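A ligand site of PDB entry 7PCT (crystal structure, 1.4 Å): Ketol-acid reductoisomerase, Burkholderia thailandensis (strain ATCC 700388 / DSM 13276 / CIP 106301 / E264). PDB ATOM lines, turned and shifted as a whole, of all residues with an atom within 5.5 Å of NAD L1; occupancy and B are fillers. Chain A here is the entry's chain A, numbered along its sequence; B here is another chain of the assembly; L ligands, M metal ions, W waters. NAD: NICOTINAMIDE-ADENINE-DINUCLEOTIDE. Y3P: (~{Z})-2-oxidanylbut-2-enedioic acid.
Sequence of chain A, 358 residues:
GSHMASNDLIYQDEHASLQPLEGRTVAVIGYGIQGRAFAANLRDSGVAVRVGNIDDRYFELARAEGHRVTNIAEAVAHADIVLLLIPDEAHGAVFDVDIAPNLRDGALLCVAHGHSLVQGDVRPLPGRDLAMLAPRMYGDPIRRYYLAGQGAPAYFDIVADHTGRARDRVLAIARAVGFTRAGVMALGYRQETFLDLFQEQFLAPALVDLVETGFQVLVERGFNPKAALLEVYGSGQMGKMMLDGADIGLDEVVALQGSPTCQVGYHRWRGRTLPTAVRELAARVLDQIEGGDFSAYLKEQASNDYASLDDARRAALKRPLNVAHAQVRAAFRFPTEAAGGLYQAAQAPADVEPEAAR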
ATOM      1  N   GLY A  30      17.244 -14.073  24.985  1.00  0.00           N
ATOM      2  CA  GLY A  30      16.485 -14.797  23.970  1.00  0.00           C
ATOM      3  C   GLY A  30      15.146 -15.254  24.494  1.00  0.00           C
ATOM      4  O   GLY A  30      14.945 -15.393  25.723  1.00  0.00           O
ATOM      5  N   TYR A  31      14.225 -15.469  23.578  1.00  0.00           N
ATOM      6  CA  TYR A  31      12.830 -15.832  23.921  1.00  0.00           C
ATOM      7  C   TYR A  31      12.305 -16.759  22.830  1.00  0.00           C
ATOM      8  O   TYR A  31      11.149 -16.670  22.443  1.00  0.00           O
ATOM      9  CB  TYR A  31      12.014 -14.550  24.137  1.00  0.00           C
ATOM     10  CG  TYR A  31      10.731 -14.770  24.891  1.00  0.00           C
ATOM     11  CD1 TYR A  31      10.742 -14.959  26.269  1.00  0.00           C
ATOM     12  CD2 TYR A  31       9.513 -14.803  24.236  1.00  0.00           C
ATOM     13  CE1 TYR A  31       9.567 -15.163  26.975  1.00  0.00           C
ATOM     14  CE2 TYR A  31       8.328 -15.018  24.931  1.00  0.00           C
ATOM     15  CZ  TYR A  31       8.354 -15.194  26.304  1.00  0.00           C
ATOM     16  OH  TYR A  31       7.194 -15.406  26.995  1.00  0.00           O
ATOM     17  N   GLY A  32      13.205 -17.582  22.295  1.00  0.00           N
ATOM     18  CA  GLY A  32      12.880 -18.556  21.257  1.00  0.00           C
ATOM     19  C   GLY A  32      12.439 -19.879  21.837  1.00  0.00           C
ATOM     20  O   GLY A  32      11.778 -19.939  22.917  1.00  0.00           O
ATOM     21  N   ILE A  33      12.786 -20.947  21.140  1.00  0.00           N
ATOM     22  CA  ILE A  33      12.318 -22.317  21.470  1.00  0.00           C
ATOM     23  C   ILE A  33      12.682 -22.598  22.940  1.00  0.00           C
ATOM     24  O   ILE A  33      11.782 -22.965  23.700  1.00  0.00           O
ATOM     25  CB  ILE A  33      12.938 -23.330  20.485  1.00  0.00           C
ATOM     26  CG1 ILE A  33      12.472 -23.061  19.047  1.00  0.00           C
ATOM     27  CG2 ILE A  33      12.624 -24.759  20.938  1.00  0.00           C
ATOM     28  CD1 ILE A  33      13.389 -23.602  17.971  1.00  0.00           C
ATOM     29  N   GLN A  34      13.934 -22.369  23.335  1.00  0.00           N
ATOM     30  CA  GLN A  34      14.371 -22.622  24.735  1.00  0.00           C
ATOM     31  C   GLN A  34      14.028 -21.404  25.612  1.00  0.00           C
ATOM     32  O   GLN A  34      13.508 -21.609  26.722  1.00  0.00           O
ATOM     33  CB  GLN A  34      15.855 -22.968  24.767  1.00  0.00           C
ATOM     34  CG  GLN A  34      16.132 -24.341  24.165  1.00  0.00           C
ATOM     35  CD  GLN A  34      15.515 -25.439  24.986  1.00  0.00           C
ATOM     36  OE1 GLN A  34      15.486 -25.367  26.213  1.00  0.00           O
ATOM     37  NE2 GLN A  34      14.936 -26.444  24.338  1.00  0.00           N
ATOM     38  N   GLY A  35      14.347 -20.191  25.182  1.00  0.00           N
ATOM     39  CA  GLY A  35      14.152 -18.988  26.007  1.00  0.00           C
ATOM     40  C   GLY A  35      12.746 -18.880  26.543  1.00  0.00           C
ATOM     41  O   GLY A  35      12.560 -18.550  27.733  1.00  0.00           O
ATOM     42  N   ASN A  53      16.452  -9.153  24.892  1.00  0.00           N
ATOM     43  CA  ASN A  53      16.206  -9.572  23.488  1.00  0.00           C
ATOM     44  C   ASN A  53      16.503  -8.393  22.560  1.00  0.00           C
ATOM     45  O   ASN A  53      16.342  -7.240  22.994  1.00  0.00           O
ATOM     46  CB  ASN A  53      14.765 -10.071  23.319  1.00  0.00           C
ATOM     47  CG  ASN A  53      14.576 -11.007  22.142  1.00  0.00           C
ATOM     48  OD1 ASN A  53      14.555 -12.224  22.320  1.00  0.00           O
ATOM     49  ND2 ASN A  53      14.399 -10.456  20.950  1.00  0.00           N
ATOM     50  N   ILE A  54      16.930  -8.696  21.331  1.00  0.00           N
ATOM     51  CA  ILE A  54      17.095  -7.686  20.246  1.00  0.00           C
ATOM     52  C   ILE A  54      15.712  -7.217  19.781  1.00  0.00           C
ATOM     53  O   ILE A  54      14.685  -7.787  20.208  1.00  0.00           O
ATOM     54  CB  ILE A  54      17.941  -8.228  19.091  1.00  0.00           C
ATOM     55  CG1 ILE A  54      17.302  -9.433  18.404  1.00  0.00           C
ATOM     56  CG2 ILE A  54      19.351  -8.530  19.579  1.00  0.00           C
ATOM     57  CD1 ILE A  54      18.052  -9.883  17.175  1.00  0.00           C
ATOM     58  N   ASP A  56      13.059  -7.545  17.625  1.00  0.00           N
ATOM     59  CA  ASP A  56      12.409  -8.490  16.673  1.00  0.00           C
ATOM     60  C   ASP A  56      11.080  -8.995  17.262  1.00  0.00           C
ATOM     61  O   ASP A  56      10.663  -8.495  18.315  1.00  0.00           O
ATOM     62  CB  ASP A  56      13.387  -9.601  16.261  1.00  0.00           C
ATOM     63  CG  ASP A  56      13.720 -10.611  17.342  1.00  0.00           C
ATOM     64  OD1 ASP A  56      13.031 -10.625  18.383  1.00  0.00           O
ATOM     65  OD2 ASP A  56      14.658 -11.385  17.129  1.00  0.00           O
ATOM     66  N   TYR A  58      10.304 -11.570  18.796  1.00  0.00           N
ATOM     67  CA  TYR A  58      10.412 -12.299  20.085  1.00  0.00           C
ATOM     68  C   TYR A  58      10.381 -11.308  21.252  1.00  0.00           C
ATOM     69  O   TYR A  58       9.894 -11.642  22.335  1.00  0.00           O
ATOM     70  CB  TYR A  58      11.686 -13.141  20.092  1.00  0.00           C
ATOM     71  CG  TYR A  58      11.762 -14.235  19.059  1.00  0.00           C
ATOM     72  CD1 TYR A  58      12.390 -14.023  17.844  1.00  0.00           C
ATOM     73  CD2 TYR A  58      11.293 -15.516  19.334  1.00  0.00           C
ATOM     74  CE1 TYR A  58      12.553 -15.055  16.930  1.00  0.00           C
ATOM     75  CE2 TYR A  58      11.445 -16.547  18.430  1.00  0.00           C
ATOM     76  CZ  TYR A  58      12.069 -16.328  17.220  1.00  0.00           C
ATOM     77  OH  TYR A  58      12.215 -17.368  16.355  1.00  0.00           O
ATOM     78  N   ILE A  72      19.611  -6.603  25.517  1.00  0.00           N
ATOM     79  CA  ILE A  72      20.415  -7.666  26.180  1.00  0.00           C
ATOM     80  C   ILE A  72      21.319  -7.050  27.252  1.00  0.00           C
ATOM     81  O   ILE A  72      21.379  -7.598  28.362  1.00  0.00           O
ATOM     82  CB  ILE A  72      21.179  -8.501  25.148  1.00  0.00           C
ATOM     83  CG1 ILE A  72      20.200  -9.294  24.270  1.00  0.00           C
ATOM     84  CG2 ILE A  72      22.170  -9.401  25.845  1.00  0.00           C
ATOM     85  CD1 ILE A  72      20.853 -10.070  23.161  1.00  0.00           C
ATOM     86  N   LEU A  84      22.116 -17.732  28.228  1.00  0.00           N
ATOM     87  CA  LEU A  84      22.319 -17.275  26.828  1.00  0.00           C
ATOM     88  C   LEU A  84      21.584 -18.231  25.883  1.00  0.00           C
ATOM     89  O   LEU A  84      22.165 -19.237  25.471  1.00  0.00           O
ATOM     90  CB  LEU A  84      23.814 -17.214  26.522  1.00  0.00           C
ATOM     91  CG  LEU A  84      24.194 -16.665  25.147  1.00  0.00           C
ATOM     92  CD1 LEU A  84      23.527 -15.319  24.881  1.00  0.00           C
ATOM     93  CD2 LEU A  84      25.709 -16.537  25.011  1.00  0.00           C
ATOM     94  N   LEU A  85      20.322 -17.926  25.575  1.00  0.00           N
ATOM     95  CA  LEU A  85      19.429 -18.817  24.802  1.00  0.00           C
ATOM     96  C   LEU A  85      19.102 -18.148  23.455  1.00  0.00           C
ATOM     97  O   LEU A  85      17.925 -17.938  23.148  1.00  0.00           O
ATOM     98  CB  LEU A  85      18.209 -19.133  25.679  1.00  0.00           C
ATOM     99  CG  LEU A  85      18.536 -19.847  26.995  1.00  0.00           C
ATOM    100  CD1 LEU A  85      17.276 -20.136  27.795  1.00  0.00           C
ATOM    101  CD2 LEU A  85      19.297 -21.155  26.756  1.00  0.00           C
ATOM    102  N   ILE A  86      20.155 -17.862  22.690  1.00  0.00           N
ATOM    103  CA  ILE A  86      20.101 -17.407  21.272  1.00  0.00           C
ATOM    104  C   ILE A  86      20.885 -18.383  20.403  1.00  0.00           C
ATOM    105  O   ILE A  86      21.641 -19.200  20.929  1.00  0.00           O
ATOM    106  CB  ILE A  86      20.590 -15.932  21.168  1.00  0.00           C
ATOM    107  CG1 ILE A  86      22.106 -15.857  21.314  1.00  0.00           C
ATOM    108  CG2 ILE A  86      19.790 -15.055  22.127  1.00  0.00           C
ATOM    109  CD1 ILE A  86      22.709 -14.467  21.168  1.00  0.00           C
ATOM    110  N   PRO A  87      20.756 -18.330  19.057  1.00  0.00           N
ATOM    111  CA  PRO A  87      21.495 -19.200  18.134  1.00  0.00           C
ATOM    112  C   PRO A  87      23.013 -19.130  18.421  1.00  0.00           C
ATOM    113  O   PRO A  87      23.565 -18.050  18.659  1.00  0.00           O
ATOM    114  CB  PRO A  87      21.102 -18.657  16.757  1.00  0.00           C
ATOM    115  CG  PRO A  87      19.711 -18.170  17.006  1.00  0.00           C
ATOM    116  CD  PRO A  87      19.840 -17.454  18.319  1.00  0.00           C
ATOM    117  N   ASP A  88      23.642 -20.302  18.405  1.00  0.00           N
ATOM    118  CA  ASP A  88      25.052 -20.500  18.805  1.00  0.00           C
ATOM    119  C   ASP A  88      25.970 -19.576  18.002  1.00  0.00           C
ATOM    120  O   ASP A  88      26.885 -19.006  18.597  1.00  0.00           O
ATOM    121  CB  ASP A  88      25.402 -21.983  18.684  1.00  0.00           C
ATOM    122  CG  ASP A  88      24.408 -22.802  19.496  1.00  0.00           C
ATOM    123  OD1 ASP A  88      24.579 -22.844  20.723  1.00  0.00           O
ATOM    124  OD2 ASP A  88      23.430 -23.303  18.898  1.00  0.00           O
ATOM    125  N   ALA A  90      25.541 -16.640  17.026  1.00  0.00           N
ATOM    126  CA  ALA A  90      25.409 -15.239  17.490  1.00  0.00           C
ATOM    127  C   ALA A  90      26.076 -15.046  18.853  1.00  0.00           C
ATOM    128  O   ALA A  90      26.166 -13.890  19.298  1.00  0.00           O
ATOM    129  CB  ALA A  90      23.954 -14.851  17.561  1.00  0.00           C
ATOM    130  N   HIS A  91      26.510 -16.116  19.515  1.00  0.00           N
ATOM    131  CA  HIS A  91      27.058 -16.033  20.894  1.00  0.00           C
ATOM    132  C   HIS A  91      28.266 -15.094  20.961  1.00  0.00           C
ATOM    133  O   HIS A  91      28.333 -14.311  21.900  1.00  0.00           O
ATOM    134  CB  HIS A  91      27.442 -17.417  21.422  1.00  0.00           C
ATOM    135  CG  HIS A  91      26.279 -18.258  21.811  1.00  0.00           C
ATOM    136  ND1 HIS A  91      26.419 -19.417  22.550  1.00  0.00           N
ATOM    137  CD2 HIS A  91      24.961 -18.136  21.547  1.00  0.00           C
ATOM    138  CE1 HIS A  91      25.235 -19.959  22.739  1.00  0.00           C
ATOM    139  NE2 HIS A  91      24.324 -19.194  22.121  1.00  0.00           N
ATOM    140  N   VAL A  94      27.503 -11.185  20.751  1.00  0.00           N
ATOM    141  CA  VAL A  94      26.635 -10.792  21.900  1.00  0.00           C
ATOM    142  C   VAL A  94      27.444 -10.916  23.193  1.00  0.00           C
ATOM    143  O   VAL A  94      27.346 -10.028  24.051  1.00  0.00           O
ATOM    144  CB  VAL A  94      25.339 -11.620  21.932  1.00  0.00           C
ATOM    145  CG1 VAL A  94      24.550 -11.415  23.220  1.00  0.00           C
ATOM    146  CG2 VAL A  94      24.491 -11.326  20.714  1.00  0.00           C
ATOM    147  N   ALA A 112      23.284 -23.371  26.757  1.00  0.00           N
ATOM    148  CA  ALA A 112      22.443 -24.594  26.665  1.00  0.00           C
ATOM    149  C   ALA A 112      22.996 -25.571  25.626  1.00  0.00           C
ATOM    150  O   ALA A 112      22.305 -26.545  25.340  1.00  0.00           O
ATOM    151  CB  ALA A 112      21.023 -24.195  26.343  1.00  0.00           C
ATOM    152  N   HIS A 113      24.215 -25.339  25.136  1.00  0.00           N
ATOM    153  CA  HIS A 113      24.938 -26.149  24.131  1.00  0.00           C
ATOM    154  C   HIS A 113      26.410 -25.781  24.222  1.00  0.00           C
ATOM    155  O   HIS A 113      26.705 -24.590  24.409  1.00  0.00           O
ATOM    156  CB  HIS A 113      24.359 -25.851  22.752  1.00  0.00           C
ATOM    157  CG  HIS A 113      24.928 -26.617  21.592  1.00  0.00           C
ATOM    158  ND1 HIS A 113      25.270 -27.972  21.636  1.00  0.00           N
ATOM    159  CD2 HIS A 113      25.033 -26.257  20.291  1.00  0.00           C
ATOM    160  CE1 HIS A 113      25.632 -28.354  20.423  1.00  0.00           C
ATOM    161  NE2 HIS A 113      25.484 -27.335  19.591  1.00  0.00           N
ATOM    162  N   ALA A 134      22.177 -28.103  29.375  1.00  0.00           N
ATOM    163  CA  ALA A 134      21.777 -28.421  27.984  1.00  0.00           C
ATOM    164  C   ALA A 134      20.595 -29.370  27.998  1.00  0.00           C
ATOM    165  O   ALA A 134      20.783 -30.582  28.191  1.00  0.00           O
ATOM    166  CB  ALA A 134      22.938 -29.029  27.250  1.00  0.00           C
ATOM    167  N   PRO A 135      19.353 -28.875  27.781  1.00  0.00           N
ATOM    168  CA  PRO A 135      18.185 -29.755  27.774  1.00  0.00           C
ATOM    169  C   PRO A 135      18.237 -30.763  26.624  1.00  0.00           C
ATOM    170  O   PRO A 135      18.778 -30.438  25.588  1.00  0.00           O
ATOM    171  CB  PRO A 135      17.016 -28.787  27.570  1.00  0.00           C
ATOM    172  CG  PRO A 135      17.544 -27.458  28.036  1.00  0.00           C
ATOM    173  CD  PRO A 135      18.989 -27.468  27.578  1.00  0.00           C
ATOM    174  N   MET A 137      15.564 -31.846  24.958  1.00  0.00           N
ATOM    175  CA  MET A 137      14.173 -31.741  24.464  1.00  0.00           C
ATOM    176  C   MET A 137      13.930 -30.308  24.023  1.00  0.00           C
ATOM    177  O   MET A 137      14.617 -29.412  24.517  1.00  0.00           O
ATOM    178  CB  MET A 137      13.222 -32.125  25.599  1.00  0.00           C
ATOM    179  CG  MET A 137      11.754 -32.119  25.254  1.00  0.00           C
ATOM    180  SD  MET A 137      11.343 -33.247  23.887  1.00  0.00           S
ATOM    181  CE  MET A 137      11.910 -34.793  24.592  1.00  0.00           C
ATOM    182  N   TYR A 138      12.974 -30.105  23.111  1.00  0.00           N
ATOM    183  CA  TYR A 138      12.606 -28.745  22.640  1.00  0.00           C
ATOM    184  C   TYR A 138      11.564 -28.140  23.573  1.00  0.00           C
ATOM    185  O   TYR A 138      11.116 -28.770  24.543  1.00  0.00           O
ATOM    186  CB  TYR A 138      12.277 -28.749  21.143  1.00  0.00           C
ATOM    187  CG  TYR A 138      11.334 -29.802  20.630  1.00  0.00           C
ATOM    188  CD1 TYR A 138       9.988 -29.542  20.472  1.00  0.00           C
ATOM    189  CD2 TYR A 138      11.816 -31.018  20.165  1.00  0.00           C
ATOM    190  CE1 TYR A 138       9.128 -30.482  19.931  1.00  0.00           C
ATOM    191  CE2 TYR A 138      10.975 -31.973  19.603  1.00  0.00           C
ATOM    192  CZ  TYR A 138       9.618 -31.697  19.486  1.00  0.00           C
ATOM    193  OH  TYR A 138       8.790 -32.628  18.938  1.00  0.00           O
ATOM    194  N   GLY A 139      11.182 -26.899  23.301  1.00  0.00           N
ATOM    195  CA  GLY A 139      10.501 -26.024  24.274  1.00  0.00           C
ATOM    196  C   GLY A 139       9.090 -26.480  24.615  1.00  0.00           C
ATOM    197  O   GLY A 139       8.768 -26.515  25.807  1.00  0.00           O
ATOM    198  N   ASP A 196      25.275 -33.932  20.561  1.00  0.00           N
ATOM    199  CA  ASP A 196      24.090 -33.174  20.122  1.00  0.00           C
ATOM    200  C   ASP A 196      24.116 -33.021  18.609  1.00  0.00           C
ATOM    201  O   ASP A 196      23.106 -33.281  17.939  1.00  0.00           O
ATOM    202  CB  ASP A 196      24.071 -31.808  20.804  1.00  0.00           C
ATOM    203  CG  ASP A 196      22.731 -31.110  20.653  1.00  0.00           C
ATOM    204  OD1 ASP A 196      21.724 -31.682  21.131  1.00  0.00           O
ATOM    205  OD2 ASP A 196      22.711 -30.039  20.064  1.00  0.00           O
ATOM    206  N   GLN B 257      11.149 -26.230  15.420  1.00  0.00           N
ATOM    207  CA  GLN B 257      11.629 -26.596  16.780  1.00  0.00           C
ATOM    208  C   GLN B 257      13.154 -26.691  16.847  1.00  0.00           C
ATOM    209  O   GLN B 257      13.666 -26.826  17.989  1.00  0.00           O
ATOM    210  CB  GLN B 257      11.031 -27.920  17.240  1.00  0.00           C
ATOM    211  CG  GLN B 257       9.499 -27.929  17.241  1.00  0.00           C
ATOM    212  CD  GLN B 257       8.878 -27.043  18.292  1.00  0.00           C
ATOM    213  OE1 GLN B 257       9.477 -26.085  18.773  1.00  0.00           O
ATOM    214  NE2 GLN B 257       7.645 -27.350  18.642  1.00  0.00           N
ATOM    215  N   GLY B 258      13.858 -26.638  15.719  1.00  0.00           N
ATOM    216  CA  GLY B 258      15.336 -26.711  15.711  1.00  0.00           C
ATOM    217  C   GLY B 258      15.944 -25.336  15.873  1.00  0.00           C
ATOM    218  O   GLY B 258      15.468 -24.371  15.224  1.00  0.00           O
ATOM    219  N   SER B 259      17.029 -25.244  16.640  1.00  0.00           N
ATOM    220  CA  SER B 259      17.937 -24.079  16.592  1.00  0.00           C
ATOM    221  C   SER B 259      18.442 -23.929  15.166  1.00  0.00           C
ATOM    222  O   SER B 259      18.458 -24.891  14.392  1.00  0.00           O
ATOM    223  CB  SER B 259      19.082 -24.251  17.559  1.00  0.00           C
ATOM    224  OG  SER B 259      20.005 -25.219  17.077  1.00  0.00           O
ATOM    225  N   PRO B 260      18.958 -22.750  14.772  1.00  0.00           N
ATOM    226  CA  PRO B 260      19.592 -22.615  13.467  1.00  0.00           C
ATOM    227  C   PRO B 260      20.756 -23.607  13.309  1.00  0.00           C
ATOM    228  O   PRO B 260      20.937 -24.149  12.232  1.00  0.00           O
ATOM    229  CB  PRO B 260      20.004 -21.133  13.438  1.00  0.00           C
ATOM    230  CG  PRO B 260      18.987 -20.474  14.375  1.00  0.00           C
ATOM    231  CD  PRO B 260      18.851 -21.470  15.498  1.00  0.00           C
ATOM    232  N   THR B 261      21.478 -23.897  14.387  1.00  0.00           N
ATOM    233  CA  THR B 261      22.589 -24.885  14.390  1.00  0.00           C
ATOM    234  C   THR B 261      22.038 -26.248  13.966  1.00  0.00           C
ATOM    235  O   THR B 261      22.617 -26.919  13.089  1.00  0.00           O
ATOM    236  CB  THR B 261      23.246 -24.971  15.773  1.00  0.00           C
ATOM    237  OG1 THR B 261      23.599 -23.633  16.163  1.00  0.00           O
ATOM    238  CG2 THR B 261      24.467 -25.864  15.772  1.00  0.00           C
HETATM  239  PA  NAD L   1      15.897 -19.868  18.395  1.00  0.00           P
HETATM  240  O1A NAD L   1      16.218 -19.974  16.947  1.00  0.00           O
HETATM  241  O2A NAD L   1      14.521 -20.189  18.886  1.00  0.00           O
HETATM  242  O5B NAD L   1      16.353 -18.457  18.936  1.00  0.00           O
HETATM  243  C5B NAD L   1      15.551 -17.304  18.706  1.00  0.00           C
HETATM  244  C4B NAD L   1      15.928 -16.272  19.727  1.00  0.00           C
HETATM  245  O4B NAD L   1      17.289 -15.827  19.484  1.00  0.00           O
HETATM  246  C3B NAD L   1      15.070 -15.014  19.741  1.00  0.00           C
HETATM  247  O3B NAD L   1      14.913 -14.546  21.073  1.00  0.00           O
HETATM  248  C2B NAD L   1      15.884 -14.058  18.883  1.00  0.00           C
HETATM  249  O2B NAD L   1      15.618 -12.705  19.178  1.00  0.00           O
HETATM  250  C1B NAD L   1      17.296 -14.440  19.298  1.00  0.00           C
HETATM  251  N9A NAD L   1      18.320 -14.119  18.319  1.00  0.00           N
HETATM  252  C8A NAD L   1      18.439 -14.614  17.044  1.00  0.00           C
HETATM  253  N7A NAD L   1      19.488 -14.152  16.422  1.00  0.00           N
HETATM  254  C5A NAD L   1      20.085 -13.269  17.309  1.00  0.00           C
HETATM  255  C6A NAD L   1      21.228 -12.445  17.231  1.00  0.00           C
HETATM  256  N6A NAD L   1      22.001 -12.338  16.153  1.00  0.00           N
HETATM  257  N1A NAD L   1      21.525 -11.685  18.318  1.00  0.00           N
HETATM  258  C2A NAD L   1      20.742 -11.782  19.395  1.00  0.00           C
HETATM  259  N3A NAD L   1      19.659 -12.529  19.591  1.00  0.00           N
HETATM  260  C4A NAD L   1      19.375 -13.259  18.494  1.00  0.00           C
HETATM  261  O3  NAD L   1      16.969 -20.732  19.205  1.00  0.00           O
HETATM  262  PN  NAD L   1      16.882 -21.960  20.246  1.00  0.00           P
HETATM  263  O1N NAD L   1      16.630 -23.221  19.495  1.00  0.00           O
HETATM  264  O2N NAD L   1      15.958 -21.588  21.348  1.00  0.00           O
HETATM  265  O5D NAD L   1      18.396 -22.038  20.724  1.00  0.00           O
HETATM  266  C5D NAD L   1      18.906 -21.281  21.821  1.00  0.00           C
HETATM  267  C4D NAD L   1      20.064 -22.049  22.422  1.00  0.00           C
HETATM  268  O4D NAD L   1      19.570 -23.288  22.985  1.00  0.00           O
HETATM  269  C3D NAD L   1      21.194 -22.473  21.485  1.00  0.00           C
HETATM  270  O3D NAD L   1      22.432 -22.451  22.200  1.00  0.00           O
HETATM  271  C2D NAD L   1      20.785 -23.903  21.099  1.00  0.00           C
HETATM  272  O2D NAD L   1      21.877 -24.687  20.647  1.00  0.00           O
HETATM  273  C1D NAD L   1      20.282 -24.386  22.449  1.00  0.00           C
HETATM  274  N1N NAD L   1      19.327 -25.535  22.446  1.00  0.00           N
HETATM  275  C2N NAD L   1      18.188 -25.522  21.672  1.00  0.00           C
HETATM  276  C3N NAD L   1      17.229 -26.516  21.803  1.00  0.00           C
HETATM  277  C7N NAD L   1      15.990 -26.551  21.018  1.00  0.00           C
HETATM  278  O7N NAD L   1      15.121 -27.365  21.368  1.00  0.00           O
HETATM  279  N7N NAD L   1      15.817 -25.777  19.954  1.00  0.00           N
HETATM  280  C4N NAD L   1      17.462 -27.598  22.783  1.00  0.00           C
HETATM  281  C5N NAD L   1      18.690 -27.521  23.528  1.00  0.00           C
HETATM  282  C6N NAD L   1      19.552 -26.550  23.342  1.00  0.00           C
HETATM  283  C1  Y3P L   2      18.789 -27.855  18.811  1.00  0.00           C
HETATM  284  O1  Y3P L   2      17.746 -27.426  18.232  1.00  0.00           O
HETATM  285  C2  Y3P L   2      18.654 -28.940  19.802  1.00  0.00           C
HETATM  286  O2  Y3P L   2      19.920 -27.416  18.607  1.00  0.00           O
HETATM  287  C3  Y3P L   2      17.283 -29.398  20.021  1.00  0.00           C
HETATM  288  O3  Y3P L   2      19.750 -29.462  20.409  1.00  0.00           O
HETATM  289  C4  Y3P L   2      16.927 -30.443  21.037  1.00  0.00           C
HETATM  290  O4  Y3P L   2      17.782 -31.038  21.754  1.00  0.00           O
HETATM  291  O5  Y3P L   2      15.696 -30.646  21.231  1.00  0.00           O
HETATM  292 MG    MG M   1      21.356 -28.738  19.307  1.00  0.00          MG
HETATM  293 MG    MG M   2      19.740 -31.325  21.308  1.00  0.00          MG
HETATM  294  O   HOH W   1      15.000 -21.679  15.218  1.00  0.00           O
HETATM  295  O   HOH W   2      22.636  -8.991  18.603  1.00  0.00           O
HETATM  296  O   HOH W   3      17.584 -11.490  21.261  1.00  0.00           O
HETATM  297  O   HOH W   4      20.605 -15.779  14.369  1.00  0.00           O
HETATM  298  O   HOH W   5      16.615 -17.659  15.417  1.00  0.00           O
HETATM  299  O   HOH W   6      21.845 -27.424  20.878  1.00  0.00           O
HETATM  300  O   HOH W   7      22.274 -28.562  23.338  1.00  0.00           O
HETATM  301  O   HOH W   8      12.254 -19.776  17.425  1.00  0.00           O
HETATM  302  O   HOH W   9      15.599 -19.269  22.767  1.00  0.00           O
HETATM  303  O   HOH W  10      23.157 -21.606  24.652  1.00  0.00           O
HETATM  304  O   HOH W  11      20.222 -30.443  23.166  1.00  0.00           O
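A nitrogen (N7N) of NAD L1 lies within hydrogen-bond range of the backbone carbonyl oxygen (O) of Gln 257 of chain B. OD1 of Asn 53 is in hydrogen-bond range of O3B of NAD L1 (2.7 Å). The side-chain carboxylate (OD2) of Asp 56 is in hydrogen-bond range of an oxygen (O2B) of NAD L1, at 2.6 Å. The backbone NH (N) of Ser 259 of chain B lies within hydrogen-bond range of an oxygen (O1) of Y3P L2, 2.8 Å away. O3D of NAD L1 sits at hydrogen-bond distance from OD1 of Asp 88 (2.6 Å). O3B of NAD L1 lies within hydrogen-bond range of N of Tyr 31, at 2.8 Å. The backbone NH (N) of Ile 33 is in hydrogen-bond range of an oxygen (O2A) of NAD L1, at 2.9 Å. N of Tyr 138 is in hydrogen-bond range of O5 of Y3P L2 (3.4 Å). N of Gln 34 lies within hydrogen-bond range of O2N of NAD L1 (2.9 Å). NE2 of Gln 34 is in hydrogen-bond range of O7N of NAD L1, 3.1 Å away. OG of Ser 259 of chain B lies within hydrogen-bond range of O1 of Y3P L2 (3.4 Å).
An oxygen (O1) of Y3P L2 lies within hydrogen-bond range of a nitrogen (N7N) of NAD L1, at 3.1 Å.
O of Ile 86 lies within hydrogen-bond range of NE2 of His 91, 2.9 Å away. OG of Ser 259 of chain B sits close to N of Thr 261 of chain B, at 3.3 Å. OD1 of Asp 56 lies within hydrogen-bond range of N of Tyr 58 (2.9 Å). ND2 of Asn 53 lies within hydrogen-bond range of OD1 of Asp 56 (2.9 Å). NE2 of Gln 34 lies within hydrogen-bond range of O of Met 137, at 3.0 Å. OD1 of Asn 53 is in hydrogen-bond range of N of Tyr 31 (3.5 Å). OG1 of Thr 261 of chain B is in hydrogen-bond range of OD2 of Asp 88.
Merely in contact with NAD L1: Gly 30 (3.3 Å), Gly 32 (3.3 Å), Ile 54 (3.5 Å), Tyr 58 (3.4 Å), Leu 85 (3.5 Å), Ile 86 (3.3 Å), Pro 87 (3.2 Å), Ala 90 (3.5 Å), His 91 (3.8 Å), Val 94 (3.8 Å), Ala 112 (3.4 Å), His 113 (3.5 Å), Pro 135 (3.6 Å), Met 137 (3.8 Å), Tyr 138 (3.1 Å), Ser 259 of chain B (3.3 Å) and Pro 260 of chain B (3.4 Å). Hydrophobic or aromatic side chains that line NAD L1: Ile 33, Ile 54, Tyr 58, Ile 86, Pro 87, Ala 90, His 91, Val 94, Ala 112, His 113, Tyr 138 and Pro 260 of chain B. Within 4 Å of NAD L1: Gly 30, Tyr 31, Gly 32, Ile 33, Gln 34, Asn 53, Ile 54, Asp 56, Tyr 58, Leu 85, Ile 86, Pro 87, Asp 88, Ala 90, His 91, Val 94, Ala 112, His 113, Pro 135, Met 137, Tyr 138, Gln 257 of chain B, Ser 259 of chain B and Pro 260 of chain B. Along chain A the residues within 4 Å of NAD L1 span positions 30 to 138. The nearest printed residue that does not touch NAD L1 is Gly 258 of chain B (4.1 Å).
Water W10 lies within hydrogen-bond range of O3D of NAD L1, O of Leu 84 and N of Ala 112. Water W1 bridges O1A of NAD L1 (2.7 Å) and O of Gly 258 of chain B (2.7 Å). Water W8 bridges OH of Tyr 58 (2.6 Å) and O2A of NAD L1 (2.7 Å). Water W9 lies within hydrogen-bond range of the backbone carbonyl oxygen of Leu 85 (2.7 Å), an oxygen (O2N) of NAD L1 (2.7 Å), the backbone NH of Gly 35 (2.9 Å) and the backbone NH of Gly 32 (3.0 Å). Water W3 lies within hydrogen-bond range of a nitrogen (N3A) of NAD L1 (2.9 Å), the backbone NH of Ile 54 (2.9 Å) and the side-chain amide oxygen of Asn 53 (3.3 Å). Water W7 bridges the backbone carbonyl oxygen (O) of Ala 112 (2.8 Å) and a ring nitrogen (ND1) of His 113 (3.5 Å).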
